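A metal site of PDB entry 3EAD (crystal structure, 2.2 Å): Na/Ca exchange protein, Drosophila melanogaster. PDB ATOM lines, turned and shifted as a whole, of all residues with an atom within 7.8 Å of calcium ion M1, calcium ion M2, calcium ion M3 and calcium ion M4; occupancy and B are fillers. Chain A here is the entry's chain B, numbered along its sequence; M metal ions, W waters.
Of the 24 residues printed, 3 come within 4 Å of calcium ion M2.
OD1 of Asp 53 binds calcium ion M4, 2.5 Å away.
The side-chain carboxylate (OE2) of Glu 83 binds calcium ion M4 (2.5 Å).
Water W1 binds calcium ion M4 (2.5 Å).
OE2 of Glu 86 is bound to calcium ion M4, at 2.6 Å.
The side-chain carboxylate (OD2) of Asp 53 is bound to calcium ion M4.
Calcium ion M4 is bound by the side-chain carboxylate (OE1) of Glu 86.
Calcium ion M4 has six donor atoms within binding distance.
Three residues have an atom within 4 Å of calcium ion M4: Asp 53, Glu 83 and Glu 86.
The nearest printed residue that does not touch calcium ion M4 is Thr 47 (4.7 Å).
Within 4 Å of calcium ion M3: Glu 18, Asp 79, Val 81, Glu 83, Asp 113 and Asp 115.
The nearest printed residue that does not touch calcium ion M3 is Asp 80 (4.7 Å).
Water W2 lies within hydrogen-bond range of O of Ile 77 (2.6 Å) and O of Asp 53 (2.7 Å).
Within 4 Å of calcium ion M1: Glu 18, Asp 78, Asp 79, Asp 114 and Asp 115.
The nearest printed residue that does not touch calcium ion M1 is Asp 80 (4.3 Å).
Calcium ion M3 is bound by OD1 of Asp 113 (2.3 Å).
OD2 of Asp 115 binds calcium ion M3 (2.3 Å).
Calcium ion M3 is bound by the side-chain carboxylate (OE1) of Glu 83 (2.5 Å).
Calcium ion M3 is bound by the backbone carbonyl oxygen (O) of Val 81 (2.5 Å).
The side-chain carboxylate (OE1) of Glu 18 binds calcium ion M3.
The side-chain carboxylate (OD2) of Asp 79 binds calcium ion M3 (2.6 Å).
The side-chain carboxylate (OE2) of Glu 18 is bound to calcium ion M3 (2.6 Å).
Calcium ion M3 has seven donor atoms within binding distance.
The backbone NH (N) of Glu 18 is in hydrogen-bond range of the backbone carbonyl oxygen (O) of Leu 112 (2.9 Å).
The backbone carbonyl oxygen of Asp 53 is in hydrogen-bond range of the backbone NH of Ile 77 (2.9 Å).
The side-chain carboxylate (OD1) of Asp 53 sits close to the backbone NH (N) of Ser 49, 3.0 Å away.
The backbone carbonyl oxygen of Glu 86 lies within hydrogen-bond range of the backbone NH of Ile 111 (2.7 Å).
Calcium ion M1 is bound by OD2 of Asp 78, O of Asp 79, OD1 of Asp 114, OD1 of Asp 115, OE2 of Glu 18 and OD2 of Asp 115.
Calcium ion M1 has six donor atoms within binding distance.
The side-chain carboxylate (OE1) of Glu 18 is bound to calcium ion M2, at 2.4 Å.
Water W3 binds calcium ion M2, at 2.5 Å.
Water W2 is bound to calcium ion M2 (2.5 Å).
Calcium ion M2 is bound by OD2 of Asp 53, 2.5 Å away.
OE2 of Glu 83 binds calcium ion M2 (2.6 Å).
The side-chain carboxylate (OE1) of Glu 83 binds calcium ion M2, at 2.7 Å.
Calcium ion M2 has six donor atoms within binding distance.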
ATOM      1  N   GLU A  18      -9.741 -20.150 -20.343  1.00  0.00           N
ATOM      2  CA  GLU A  18      -9.806 -20.772 -21.667  1.00  0.00           C
ATOM      3  C   GLU A  18     -11.226 -20.940 -22.238  1.00  0.00           C
ATOM      4  O   GLU A  18     -11.480 -20.806 -23.450  1.00  0.00           O
ATOM      5  CB  GLU A  18      -9.084 -22.130 -21.651  1.00  0.00           C
ATOM      6  CG  GLU A  18      -8.956 -22.689 -23.028  1.00  0.00           C
ATOM      7  CD  GLU A  18      -8.457 -24.105 -23.041  1.00  0.00           C
ATOM      8  OE1 GLU A  18      -7.403 -24.349 -23.660  1.00  0.00           O
ATOM      9  OE2 GLU A  18      -9.109 -24.983 -22.445  1.00  0.00           O
ATOM     10  N   ASN A  19     -12.154 -21.244 -21.376  1.00  0.00           N
ATOM     11  CA  ASN A  19     -13.522 -21.427 -21.831  1.00  0.00           C
ATOM     12  C   ASN A  19     -14.264 -20.102 -21.961  1.00  0.00           C
ATOM     13  O   ASN A  19     -15.483 -20.110 -22.063  1.00  0.00           O
ATOM     14  CB  ASN A  19     -14.275 -22.397 -20.910  1.00  0.00           C
ATOM     15  CG  ASN A  19     -14.397 -21.885 -19.477  1.00  0.00           C
ATOM     16  OD1 ASN A  19     -13.441 -21.382 -18.898  1.00  0.00           O
ATOM     17  ND2 ASN A  19     -15.592 -22.030 -18.904  1.00  0.00           N
ATOM     18  N   THR A  47       3.604 -18.630 -25.916  1.00  0.00           N
ATOM     19  CA  THR A  47       3.662 -20.070 -25.656  1.00  0.00           C
ATOM     20  C   THR A  47       2.321 -20.651 -26.039  1.00  0.00           C
ATOM     21  O   THR A  47       2.191 -21.861 -26.231  1.00  0.00           O
ATOM     22  CB  THR A  47       4.016 -20.437 -24.216  1.00  0.00           C
ATOM     23  OG1 THR A  47       3.243 -19.656 -23.295  1.00  0.00           O
ATOM     24  CG2 THR A  47       5.496 -20.260 -23.959  1.00  0.00           C
ATOM     25  N   ALA A  48       1.316 -19.771 -26.161  1.00  0.00           N
ATOM     26  CA  ALA A  48       0.028 -20.050 -26.783  1.00  0.00           C
ATOM     27  C   ALA A  48       0.076 -19.728 -28.288  1.00  0.00           C
ATOM     28  O   ALA A  48       0.742 -18.786 -28.717  1.00  0.00           O
ATOM     29  CB  ALA A  48      -1.017 -19.224 -26.125  1.00  0.00           C
ATOM     30  N   SER A  49      -0.664 -20.493 -29.086  1.00  0.00           N
ATOM     31  CA  SER A  49      -0.586 -20.329 -30.522  1.00  0.00           C
ATOM     32  C   SER A  49      -1.900 -20.042 -31.241  1.00  0.00           C
ATOM     33  O   SER A  49      -2.955 -20.539 -30.857  1.00  0.00           O
ATOM     34  CB  SER A  49       0.140 -21.494 -31.139  1.00  0.00           C
ATOM     35  OG  SER A  49       1.420 -21.555 -30.544  1.00  0.00           O
ATOM     36  N   THR A  52      -4.626 -22.959 -32.185  1.00  0.00           N
ATOM     37  CA  THR A  52      -4.882 -23.930 -31.118  1.00  0.00           C
ATOM     38  C   THR A  52      -5.277 -23.315 -29.751  1.00  0.00           C
ATOM     39  O   THR A  52      -5.948 -23.967 -28.939  1.00  0.00           O
ATOM     40  CB  THR A  52      -3.699 -24.851 -30.924  1.00  0.00           C
ATOM     41  OG1 THR A  52      -2.502 -24.072 -31.000  1.00  0.00           O
ATOM     42  CG2 THR A  52      -3.693 -25.882 -31.997  1.00  0.00           C
ATOM     43  N   ASP A  53      -4.881 -22.080 -29.506  1.00  0.00           N
ATOM     44  CA  ASP A  53      -5.213 -21.453 -28.227  1.00  0.00           C
ATOM     45  C   ASP A  53      -6.084 -20.208 -28.330  1.00  0.00           C
ATOM     46  O   ASP A  53      -6.918 -19.945 -27.444  1.00  0.00           O
ATOM     47  CB  ASP A  53      -3.937 -21.208 -27.458  1.00  0.00           C
ATOM     48  CG  ASP A  53      -3.216 -22.513 -27.133  1.00  0.00           C
ATOM     49  OD1 ASP A  53      -2.006 -22.621 -27.384  1.00  0.00           O
ATOM     50  OD2 ASP A  53      -3.896 -23.431 -26.615  1.00  0.00           O
ATOM     51  N   PHE A  54      -5.879 -19.456 -29.416  1.00  0.00           N
ATOM     52  CA  PHE A  54      -6.712 -18.325 -29.747  1.00  0.00           C
ATOM     53  C   PHE A  54      -6.794 -18.292 -31.261  1.00  0.00           C
ATOM     54  O   PHE A  54      -6.085 -19.065 -31.961  1.00  0.00           O
ATOM     55  CB  PHE A  54      -6.104 -17.016 -29.186  1.00  0.00           C
ATOM     56  CG  PHE A  54      -4.749 -16.673 -29.782  1.00  0.00           C
ATOM     57  CD1 PHE A  54      -3.636 -17.452 -29.493  1.00  0.00           C
ATOM     58  CD2 PHE A  54      -4.610 -15.608 -30.674  1.00  0.00           C
ATOM     59  CE1 PHE A  54      -2.399 -17.146 -30.049  1.00  0.00           C
ATOM     60  CE2 PHE A  54      -3.384 -15.308 -31.249  1.00  0.00           C
ATOM     61  CZ  PHE A  54      -2.273 -16.084 -30.943  1.00  0.00           C
ATOM     62  N   VAL A  76     -10.959 -16.994 -27.960  1.00  0.00           N
ATOM     63  CA  VAL A  76     -10.126 -17.993 -27.292  1.00  0.00           C
ATOM     64  C   VAL A  76     -10.661 -19.400 -27.588  1.00  0.00           C
ATOM     65  O   VAL A  76     -11.868 -19.674 -27.466  1.00  0.00           O
ATOM     66  CB  VAL A  76      -9.986 -17.712 -25.764  1.00  0.00           C
ATOM     67  CG1 VAL A  76      -9.084 -18.713 -25.052  1.00  0.00           C
ATOM     68  CG2 VAL A  76      -9.360 -16.338 -25.592  1.00  0.00           C
ATOM     69  N   ILE A  77      -9.733 -20.251 -28.008  1.00  0.00           N
ATOM     70  CA  ILE A  77     -10.078 -21.565 -28.474  1.00  0.00           C
ATOM     71  C   ILE A  77     -10.064 -22.512 -27.300  1.00  0.00           C
ATOM     72  O   ILE A  77      -9.026 -22.737 -26.681  1.00  0.00           O
ATOM     73  CB  ILE A  77      -9.103 -22.084 -29.560  1.00  0.00           C
ATOM     74  CG1 ILE A  77      -9.112 -21.138 -30.781  1.00  0.00           C
ATOM     75  CG2 ILE A  77      -9.453 -23.525 -29.974  1.00  0.00           C
ATOM     76  CD1 ILE A  77      -8.102 -21.537 -31.838  1.00  0.00           C
ATOM     77  N   ASP A  78     -11.237 -23.066 -27.009  1.00  0.00           N
ATOM     78  CA  ASP A  78     -11.396 -24.040 -25.952  1.00  0.00           C
ATOM     79  C   ASP A  78     -11.297 -25.495 -26.472  1.00  0.00           C
ATOM     80  O   ASP A  78     -11.882 -25.834 -27.501  1.00  0.00           O
ATOM     81  CB  ASP A  78     -12.737 -23.812 -25.267  1.00  0.00           C
ATOM     82  CG  ASP A  78     -12.841 -24.523 -23.933  1.00  0.00           C
ATOM     83  OD1 ASP A  78     -13.957 -24.561 -23.376  1.00  0.00           O
ATOM     84  OD2 ASP A  78     -11.812 -25.042 -23.443  1.00  0.00           O
ATOM     85  N   ASP A  79     -10.539 -26.343 -25.759  1.00  0.00           N
ATOM     86  CA  ASP A  79     -10.523 -27.791 -26.012  1.00  0.00           C
ATOM     87  C   ASP A  79     -10.556 -28.558 -24.688  1.00  0.00           C
ATOM     88  O   ASP A  79     -11.020 -28.017 -23.677  1.00  0.00           O
ATOM     89  CB  ASP A  79      -9.312 -28.219 -26.860  1.00  0.00           C
ATOM     90  CG  ASP A  79      -7.978 -27.702 -26.313  1.00  0.00           C
ATOM     91  OD1 ASP A  79      -7.114 -27.320 -27.138  1.00  0.00           O
ATOM     92  OD2 ASP A  79      -7.782 -27.648 -25.078  1.00  0.00           O
ATOM     93  N   ASP A  80     -10.025 -29.791 -24.714  1.00  0.00           N
ATOM     94  CA  ASP A  80     -10.095 -30.785 -23.637  1.00  0.00           C
ATOM     95  C   ASP A  80      -8.729 -31.168 -23.100  1.00  0.00           C
ATOM     96  O   ASP A  80      -8.626 -31.976 -22.159  1.00  0.00           O
ATOM     97  CB  ASP A  80     -10.712 -32.058 -24.181  1.00  0.00           C
ATOM     98  CG  ASP A  80     -12.193 -31.994 -24.223  1.00  0.00           C
ATOM     99  OD1 ASP A  80     -12.805 -33.046 -24.477  1.00  0.00           O
ATOM    100  OD2 ASP A  80     -12.740 -30.891 -23.991  1.00  0.00           O
ATOM    101  N   VAL A  81      -7.697 -30.664 -23.743  1.00  0.00           N
ATOM    102  CA  VAL A  81      -6.340 -31.014 -23.361  1.00  0.00           C
ATOM    103  C   VAL A  81      -5.985 -30.163 -22.126  1.00  0.00           C
ATOM    104  O   VAL A  81      -6.249 -28.950 -22.097  1.00  0.00           O
ATOM    105  CB  VAL A  81      -5.380 -30.780 -24.579  1.00  0.00           C
ATOM    106  CG1 VAL A  81      -3.910 -30.987 -24.197  1.00  0.00           C
ATOM    107  CG2 VAL A  81      -5.785 -31.665 -25.743  1.00  0.00           C
ATOM    108  N   PHE A  82      -5.455 -30.823 -21.111  1.00  0.00           N
ATOM    109  CA  PHE A  82      -4.871 -30.143 -19.962  1.00  0.00           C
ATOM    110  C   PHE A  82      -3.669 -29.338 -20.421  1.00  0.00           C
ATOM    111  O   PHE A  82      -2.763 -29.871 -21.087  1.00  0.00           O
ATOM    112  CB  PHE A  82      -4.409 -31.141 -18.886  1.00  0.00           C
ATOM    113  CG  PHE A  82      -3.508 -30.535 -17.836  1.00  0.00           C
ATOM    114  CD1 PHE A  82      -2.155 -30.878 -17.776  1.00  0.00           C
ATOM    115  CD2 PHE A  82      -4.002 -29.571 -16.932  1.00  0.00           C
ATOM    116  CE1 PHE A  82      -1.317 -30.312 -16.828  1.00  0.00           C
ATOM    117  CE2 PHE A  82      -3.175 -28.991 -15.970  1.00  0.00           C
ATOM    118  CZ  PHE A  82      -1.830 -29.355 -15.919  1.00  0.00           C
ATOM    119  N   GLU A  83      -3.642 -28.061 -20.059  1.00  0.00           N
ATOM    120  CA  GLU A  83      -2.512 -27.201 -20.407  1.00  0.00           C
ATOM    121  C   GLU A  83      -2.033 -26.397 -19.218  1.00  0.00           C
ATOM    122  O   GLU A  83      -2.822 -26.038 -18.344  1.00  0.00           O
ATOM    123  CB  GLU A  83      -2.877 -26.260 -21.548  1.00  0.00           C
ATOM    124  CG  GLU A  83      -3.125 -26.936 -22.886  1.00  0.00           C
ATOM    125  CD  GLU A  83      -3.843 -26.016 -23.838  1.00  0.00           C
ATOM    126  OE1 GLU A  83      -5.057 -26.189 -24.073  1.00  0.00           O
ATOM    127  OE2 GLU A  83      -3.184 -25.081 -24.331  1.00  0.00           O
ATOM    128  N   GLU A  84      -0.737 -26.112 -19.212  1.00  0.00           N
ATOM    129  CA  GLU A  84      -0.179 -25.145 -18.268  1.00  0.00           C
ATOM    130  C   GLU A  84      -0.620 -23.741 -18.724  1.00  0.00           C
ATOM    131  O   GLU A  84      -1.122 -23.579 -19.843  1.00  0.00           O
ATOM    132  CB  GLU A  84       1.347 -25.305 -18.161  1.00  0.00           C
ATOM    133  CG  GLU A  84       1.803 -26.597 -17.416  1.00  0.00           C
ATOM    134  CD  GLU A  84       3.327 -26.852 -17.451  1.00  0.00           C
ATOM    135  OE1 GLU A  84       4.034 -26.134 -18.188  1.00  0.00           O
ATOM    136  OE2 GLU A  84       3.815 -27.761 -16.738  1.00  0.00           O
ATOM    137  N   GLU A  86      -0.545 -20.263 -20.445  1.00  0.00           N
ATOM    138  CA  GLU A  86       0.140 -19.841 -21.668  1.00  0.00           C
ATOM    139  C   GLU A  86      -0.137 -18.400 -22.010  1.00  0.00           C
ATOM    140  O   GLU A  86      -1.214 -17.871 -21.715  1.00  0.00           O
ATOM    141  CB  GLU A  86      -0.286 -20.685 -22.861  1.00  0.00           C
ATOM    142  CG  GLU A  86       0.111 -22.167 -22.787  1.00  0.00           C
ATOM    143  CD  GLU A  86      -0.474 -22.974 -23.930  1.00  0.00           C
ATOM    144  OE1 GLU A  86      -1.216 -22.399 -24.778  1.00  0.00           O
ATOM    145  OE2 GLU A  86      -0.210 -24.200 -24.003  1.00  0.00           O
ATOM    146  N   ILE A 111      -3.663 -17.054 -20.861  1.00  0.00           N
ATOM    147  CA  ILE A 111      -4.770 -18.011 -20.764  1.00  0.00           C
ATOM    148  C   ILE A 111      -4.566 -19.018 -19.620  1.00  0.00           C
ATOM    149  O   ILE A 111      -3.521 -19.658 -19.508  1.00  0.00           O
ATOM    150  CB  ILE A 111      -5.014 -18.747 -22.090  1.00  0.00           C
ATOM    151  CG1 ILE A 111      -4.977 -17.790 -23.284  1.00  0.00           C
ATOM    152  CG2 ILE A 111      -6.349 -19.473 -22.066  1.00  0.00           C
ATOM    153  CD1 ILE A 111      -4.551 -18.501 -24.671  1.00  0.00           C
ATOM    154  N   LEU A 112      -5.575 -19.130 -18.757  1.00  0.00           N
ATOM    155  CA  LEU A 112      -5.574 -20.136 -17.709  1.00  0.00           C
ATOM    156  C   LEU A 112      -6.437 -21.274 -18.198  1.00  0.00           C
ATOM    157  O   LEU A 112      -7.589 -21.049 -18.607  1.00  0.00           O
ATOM    158  CB  LEU A 112      -6.065 -19.568 -16.369  1.00  0.00           C
ATOM    159  CG  LEU A 112      -5.389 -18.229 -16.013  1.00  0.00           C
ATOM    160  CD1 LEU A 112      -5.990 -17.581 -14.791  1.00  0.00           C
ATOM    161  CD2 LEU A 112      -3.868 -18.422 -15.835  1.00  0.00           C
ATOM    162  N   ASP A 113      -5.857 -22.477 -18.212  1.00  0.00           N
ATOM    163  CA  ASP A 113      -6.494 -23.693 -18.669  1.00  0.00           C
ATOM    164  C   ASP A 113      -7.523 -24.153 -17.666  1.00  0.00           C
ATOM    165  O   ASP A 113      -7.381 -23.883 -16.467  1.00  0.00           O
ATOM    166  CB  ASP A 113      -5.437 -24.765 -18.818  1.00  0.00           C
ATOM    167  CG  ASP A 113      -5.943 -26.010 -19.537  1.00  0.00           C
ATOM    168  OD1 ASP A 113      -6.262 -25.915 -20.750  1.00  0.00           O
ATOM    169  OD2 ASP A 113      -5.961 -27.100 -18.897  1.00  0.00           O
ATOM    170  N   ASP A 114      -8.545 -24.848 -18.158  1.00  0.00           N
ATOM    171  CA  ASP A 114      -9.679 -25.323 -17.338  1.00  0.00           C
ATOM    172  C   ASP A 114      -9.861 -26.848 -17.436  1.00  0.00           C
ATOM    173  O   ASP A 114     -10.952 -27.391 -17.196  1.00  0.00           O
ATOM    174  CB  ASP A 114     -10.974 -24.572 -17.722  1.00  0.00           C
ATOM    175  CG  ASP A 114     -11.499 -24.938 -19.112  1.00  0.00           C
ATOM    176  OD1 ASP A 114     -10.680 -25.342 -19.967  1.00  0.00           O
ATOM    177  OD2 ASP A 114     -12.733 -24.834 -19.349  1.00  0.00           O
ATOM    178  N   ASP A 115      -8.794 -27.544 -17.767  1.00  0.00           N
ATOM    179  CA  ASP A 115      -8.883 -28.979 -18.012  1.00  0.00           C
ATOM    180  C   ASP A 115      -8.163 -29.798 -16.931  1.00  0.00           C
ATOM    181  O   ASP A 115      -7.183 -29.333 -16.354  1.00  0.00           O
ATOM    182  CB  ASP A 115      -8.433 -29.269 -19.445  1.00  0.00           C
ATOM    183  CG  ASP A 115      -9.185 -28.399 -20.457  1.00  0.00           C
ATOM    184  OD1 ASP A 115     -10.428 -28.482 -20.506  1.00  0.00           O
ATOM    185  OD2 ASP A 115      -8.584 -27.599 -21.188  1.00  0.00           O
ATOM    186  N   HIS A 116      -8.697 -30.990 -16.622  1.00  0.00           N
ATOM    187  CA  HIS A 116      -8.427 -31.612 -15.316  1.00  0.00           C
ATOM    188  C   HIS A 116      -7.304 -32.652 -15.297  1.00  0.00           C
ATOM    189  O   HIS A 116      -7.485 -33.753 -14.752  1.00  0.00           O
ATOM    190  CB  HIS A 116      -9.724 -32.158 -14.687  1.00  0.00           C
ATOM    191  CG  HIS A 116     -10.815 -31.139 -14.515  1.00  0.00           C
ATOM    192  ND1 HIS A 116     -12.160 -31.472 -14.494  1.00  0.00           N
ATOM    193  CD2 HIS A 116     -10.760 -29.785 -14.336  1.00  0.00           C
ATOM    194  CE1 HIS A 116     -12.876 -30.374 -14.324  1.00  0.00           C
ATOM    195  NE2 HIS A 116     -12.056 -29.346 -14.223  1.00  0.00           N
HETATM  196 CA    CA M   1     -11.053 -26.552 -22.002  1.00  0.00          CA
HETATM  197 CA    CA M   2      -5.324 -23.559 -24.548  1.00  0.00          CA
HETATM  198 CA    CA M   3      -7.117 -26.687 -22.740  1.00  0.00          CA
HETATM  199 CA    CA M   4      -1.591 -24.710 -26.163  1.00  0.00          CA
HETATM  200  O   HOH W   1      -0.500 -26.926 -25.619  1.00  0.00           O
HETATM  201  O   HOH W   2      -6.865 -21.812 -25.470  1.00  0.00           O
HETATM  202  O   HOH W   3      -3.866 -21.795 -23.568  1.00  0.00           O
